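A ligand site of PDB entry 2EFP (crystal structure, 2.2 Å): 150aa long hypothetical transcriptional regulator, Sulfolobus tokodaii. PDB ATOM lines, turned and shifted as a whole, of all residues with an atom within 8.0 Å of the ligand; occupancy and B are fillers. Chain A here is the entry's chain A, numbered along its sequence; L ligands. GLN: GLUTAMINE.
The side-chain carboxylate (OD1) of Asp 21 lies within salt-bridge range of the side-chain amino group (NZ) of Lys 31 (2.5 Å). N of Ile 29 lies within hydrogen-bond range of O of Ala 24 (3.1 Å).
Merely in contact with the ligand: Ala 24 and Pro 30. Hydrophobic or aromatic side chains that line the ligand: Ala 24 and Pro 30.
N of Ser 32 sits at hydrogen-bond distance from OXT of the ligand (3.2 Å). An oxygen (OXT) of the ligand lies within hydrogen-bond range of the side-chain hydroxyl of Ser 32 (2.6 Å). An oxygen (OE1) of the ligand lies within hydrogen-bond range of the backbone NH (N) of Lys 31, at 3.1 Å.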
ATOM      1  N   LEU A  20     -31.986 -10.826   7.636  1.00  0.00           N
ATOM      2  CA  LEU A  20     -30.745 -10.091   7.820  1.00  0.00           C
ATOM      3  C   LEU A  20     -29.579 -10.962   7.350  1.00  0.00           C
ATOM      4  O   LEU A  20     -28.587 -10.465   6.807  1.00  0.00           O
ATOM      5  CB  LEU A  20     -30.556  -9.717   9.299  1.00  0.00           C
ATOM      6  CG  LEU A  20     -31.520  -8.708   9.926  1.00  0.00           C
ATOM      7  CD1 LEU A  20     -31.442  -7.384   9.178  1.00  0.00           C
ATOM      8  CD2 LEU A  20     -32.941  -9.254   9.895  1.00  0.00           C
ATOM      9  N   ASP A  21     -29.713 -12.276   7.546  1.00  0.00           N
ATOM     10  CA  ASP A  21     -28.690 -13.228   7.142  1.00  0.00           C
ATOM     11  C   ASP A  21     -28.452 -13.188   5.644  1.00  0.00           C
ATOM     12  O   ASP A  21     -27.325 -12.994   5.188  1.00  0.00           O
ATOM     13  CB  ASP A  21     -29.091 -14.647   7.526  1.00  0.00           C
ATOM     14  CG  ASP A  21     -29.089 -14.873   9.013  1.00  0.00           C
ATOM     15  OD1 ASP A  21     -29.947 -14.280   9.694  1.00  0.00           O
ATOM     16  OD2 ASP A  21     -28.231 -15.638   9.481  1.00  0.00           O
ATOM     17  N   GLU A  22     -29.515 -13.393   4.885  1.00  0.00           N
ATOM     18  CA  GLU A  22     -29.433 -13.396   3.439  1.00  0.00           C
ATOM     19  C   GLU A  22     -28.803 -12.134   2.895  1.00  0.00           C
ATOM     20  O   GLU A  22     -27.975 -12.182   1.978  1.00  0.00           O
ATOM     21  CB  GLU A  22     -30.826 -13.592   2.840  1.00  0.00           C
ATOM     22  CG  GLU A  22     -31.448 -14.933   3.160  1.00  0.00           C
ATOM     23  CD  GLU A  22     -32.847 -15.073   2.617  1.00  0.00           C
ATOM     24  OE1 GLU A  22     -33.737 -14.299   3.042  1.00  0.00           O
ATOM     25  OE2 GLU A  22     -33.059 -15.962   1.750  1.00  0.00           O
ATOM     26  N   ILE A  23     -29.191 -10.992   3.455  1.00  0.00           N
ATOM     27  CA  ILE A  23     -28.656  -9.709   3.004  1.00  0.00           C
ATOM     28  C   ILE A  23     -27.208  -9.554   3.479  1.00  0.00           C
ATOM     29  O   ILE A  23     -26.330  -9.180   2.696  1.00  0.00           O
ATOM     30  CB  ILE A  23     -29.504  -8.530   3.525  1.00  0.00           C
ATOM     31  CG1 ILE A  23     -30.954  -8.690   3.037  1.00  0.00           C
ATOM     32  CG2 ILE A  23     -28.936  -7.215   3.024  1.00  0.00           C
ATOM     33  CD1 ILE A  23     -31.898  -7.649   3.554  1.00  0.00           C
ATOM     34  N   ALA A  24     -26.970  -9.841   4.759  1.00  0.00           N
ATOM     35  CA  ALA A  24     -25.627  -9.738   5.319  1.00  0.00           C
ATOM     36  C   ALA A  24     -24.649 -10.612   4.534  1.00  0.00           C
ATOM     37  O   ALA A  24     -23.529 -10.192   4.233  1.00  0.00           O
ATOM     38  CB  ALA A  24     -25.648 -10.162   6.777  1.00  0.00           C
ATOM     39  N   ARG A  25     -25.078 -11.821   4.208  1.00  0.00           N
ATOM     40  CA  ARG A  25     -24.249 -12.759   3.466  1.00  0.00           C
ATOM     41  C   ARG A  25     -24.002 -12.302   2.027  1.00  0.00           C
ATOM     42  O   ARG A  25     -22.934 -12.550   1.462  1.00  0.00           O
ATOM     43  CB  ARG A  25     -24.905 -14.160   3.460  1.00  0.00           C
ATOM     44  CG  ARG A  25     -24.165 -15.193   2.587  1.00  0.00           C
ATOM     45  CD  ARG A  25     -24.559 -16.649   2.901  1.00  0.00           C
ATOM     46  NE  ARG A  25     -25.967 -16.936   2.644  1.00  0.00           N
ATOM     47  CZ  ARG A  25     -26.926 -16.929   3.569  1.00  0.00           C
ATOM     48  NH1 ARG A  25     -26.634 -16.664   4.835  1.00  0.00           N
ATOM     49  NH2 ARG A  25     -28.180 -17.211   3.230  1.00  0.00           N
ATOM     50  N   ARG A  28     -21.772  -9.097   2.190  1.00  0.00           N
ATOM     51  CA  ARG A  28     -20.528  -9.435   2.896  1.00  0.00           C
ATOM     52  C   ARG A  28     -20.174  -8.600   4.140  1.00  0.00           C
ATOM     53  O   ARG A  28     -19.023  -8.232   4.329  1.00  0.00           O
ATOM     54  CB  ARG A  28     -19.359  -9.383   1.904  1.00  0.00           C
ATOM     55  CG  ARG A  28     -18.936 -10.729   1.337  1.00  0.00           C
ATOM     56  CD  ARG A  28     -20.116 -11.554   0.839  1.00  0.00           C
ATOM     57  NE  ARG A  28     -19.718 -12.838   0.275  1.00  0.00           N
ATOM     58  CZ  ARG A  28     -19.003 -13.760   0.924  1.00  0.00           C
ATOM     59  NH1 ARG A  28     -18.597 -13.538   2.166  1.00  0.00           N
ATOM     60  NH2 ARG A  28     -18.690 -14.896   0.328  1.00  0.00           N
ATOM     61  N   ILE A  29     -21.153  -8.331   4.983  1.00  0.00           N
ATOM     62  CA  ILE A  29     -20.904  -7.583   6.219  1.00  0.00           C
ATOM     63  C   ILE A  29     -21.635  -8.265   7.361  1.00  0.00           C
ATOM     64  O   ILE A  29     -22.580  -9.025   7.130  1.00  0.00           O
ATOM     65  CB  ILE A  29     -21.385  -6.123   6.121  1.00  0.00           C
ATOM     66  CG1 ILE A  29     -22.910  -6.084   6.059  1.00  0.00           C
ATOM     67  CG2 ILE A  29     -20.762  -5.440   4.920  1.00  0.00           C
ATOM     68  CD1 ILE A  29     -23.486  -4.703   6.272  1.00  0.00           C
ATOM     69  N   PRO A  30     -21.220  -8.008   8.610  1.00  0.00           N
ATOM     70  CA  PRO A  30     -21.864  -8.622   9.779  1.00  0.00           C
ATOM     71  C   PRO A  30     -23.323  -8.218   9.949  1.00  0.00           C
ATOM     72  O   PRO A  30     -23.679  -7.058   9.768  1.00  0.00           O
ATOM     73  CB  PRO A  30     -20.970  -8.171  10.936  1.00  0.00           C
ATOM     74  CG  PRO A  30     -20.446  -6.879  10.468  1.00  0.00           C
ATOM     75  CD  PRO A  30     -20.104  -7.141   9.031  1.00  0.00           C
ATOM     76  N   LYS A  31     -24.157  -9.179  10.333  1.00  0.00           N
ATOM     77  CA  LYS A  31     -25.585  -8.924  10.506  1.00  0.00           C
ATOM     78  C   LYS A  31     -25.900  -7.755  11.437  1.00  0.00           C
ATOM     79  O   LYS A  31     -26.872  -7.030  11.215  1.00  0.00           O
ATOM     80  CB  LYS A  31     -26.294 -10.174  11.019  1.00  0.00           C
ATOM     81  CG  LYS A  31     -27.812 -10.034  11.045  1.00  0.00           C
ATOM     82  CD  LYS A  31     -28.402 -10.610  12.321  1.00  0.00           C
ATOM     83  CE  LYS A  31     -28.431 -12.127  12.312  1.00  0.00           C
ATOM     84  NZ  LYS A  31     -29.564 -12.693  11.521  1.00  0.00           N
ATOM     85  N   SER A  32     -25.096  -7.565  12.470  1.00  0.00           N
ATOM     86  CA  SER A  32     -25.333  -6.477  13.415  1.00  0.00           C
ATOM     87  C   SER A  32     -25.028  -5.111  12.805  1.00  0.00           C
ATOM     88  O   SER A  32     -25.661  -4.120  13.136  1.00  0.00           O
ATOM     89  CB  SER A  32     -24.515  -6.684  14.695  1.00  0.00           C
ATOM     90  OG  SER A  32     -23.134  -6.537  14.449  1.00  0.00           O
ATOM     91  N   THR A  33     -24.044  -5.063  11.915  1.00  0.00           N
ATOM     92  CA  THR A  33     -23.684  -3.813  11.251  1.00  0.00           C
ATOM     93  C   THR A  33     -24.800  -3.457  10.268  1.00  0.00           C
ATOM     94  O   THR A  33     -25.159  -2.285  10.106  1.00  0.00           O
ATOM     95  CB  THR A  33     -22.351  -3.962  10.484  1.00  0.00           C
ATOM     96  OG1 THR A  33     -21.329  -4.325  11.408  1.00  0.00           O
ATOM     97  CG2 THR A  33     -21.961  -2.652   9.822  1.00  0.00           C
ATOM     98  N   LEU A  34     -25.337  -4.472   9.609  1.00  0.00           N
ATOM     99  CA  LEU A  34     -26.425  -4.297   8.658  1.00  0.00           C
ATOM    100  C   LEU A  34     -27.646  -3.753   9.397  1.00  0.00           C
ATOM    101  O   LEU A  34     -28.230  -2.739   9.013  1.00  0.00           O
ATOM    102  CB  LEU A  34     -26.758  -5.640   8.009  1.00  0.00           C
ATOM    103  CG  LEU A  34     -28.036  -5.725   7.182  1.00  0.00           C
ATOM    104  CD1 LEU A  34     -27.902  -4.819   5.970  1.00  0.00           C
ATOM    105  CD2 LEU A  34     -28.276  -7.169   6.767  1.00  0.00           C
ATOM    106  N   SER A  35     -28.023  -4.456  10.457  1.00  0.00           N
ATOM    107  CA  SER A  35     -29.174  -4.057  11.244  1.00  0.00           C
ATOM    108  C   SER A  35     -29.041  -2.606  11.689  1.00  0.00           C
ATOM    109  O   SER A  35     -30.003  -1.848  11.668  1.00  0.00           O
ATOM    110  CB  SER A  35     -29.329  -4.974  12.463  1.00  0.00           C
ATOM    111  OG  SER A  35     -30.486  -4.624  13.194  1.00  0.00           O
HETATM  112  N   GLN L   1     -20.781 -11.282  14.201  1.00  0.00           N
HETATM  113  CA  GLN L   1     -21.873 -11.087  13.211  1.00  0.00           C
HETATM  114  C   GLN L   1     -22.735  -9.898  13.614  1.00  0.00           C
HETATM  115  O   GLN L   1     -23.857 -10.128  14.123  1.00  0.00           O
HETATM  116  CB  GLN L   1     -22.751 -12.336  13.118  1.00  0.00           C
HETATM  117  CG  GLN L   1     -23.859 -12.277  12.063  1.00  0.00           C
HETATM  118  CD  GLN L   1     -23.317 -12.219  10.631  1.00  0.00           C
HETATM  119  OE1 GLN L   1     -24.080 -12.236   9.666  1.00  0.00           O
HETATM  120  NE2 GLN L   1     -21.991 -12.145  10.502  1.00  0.00           N
HETATM  121  OXT GLN L   1     -22.274  -8.751  13.433  1.00  0.00           O
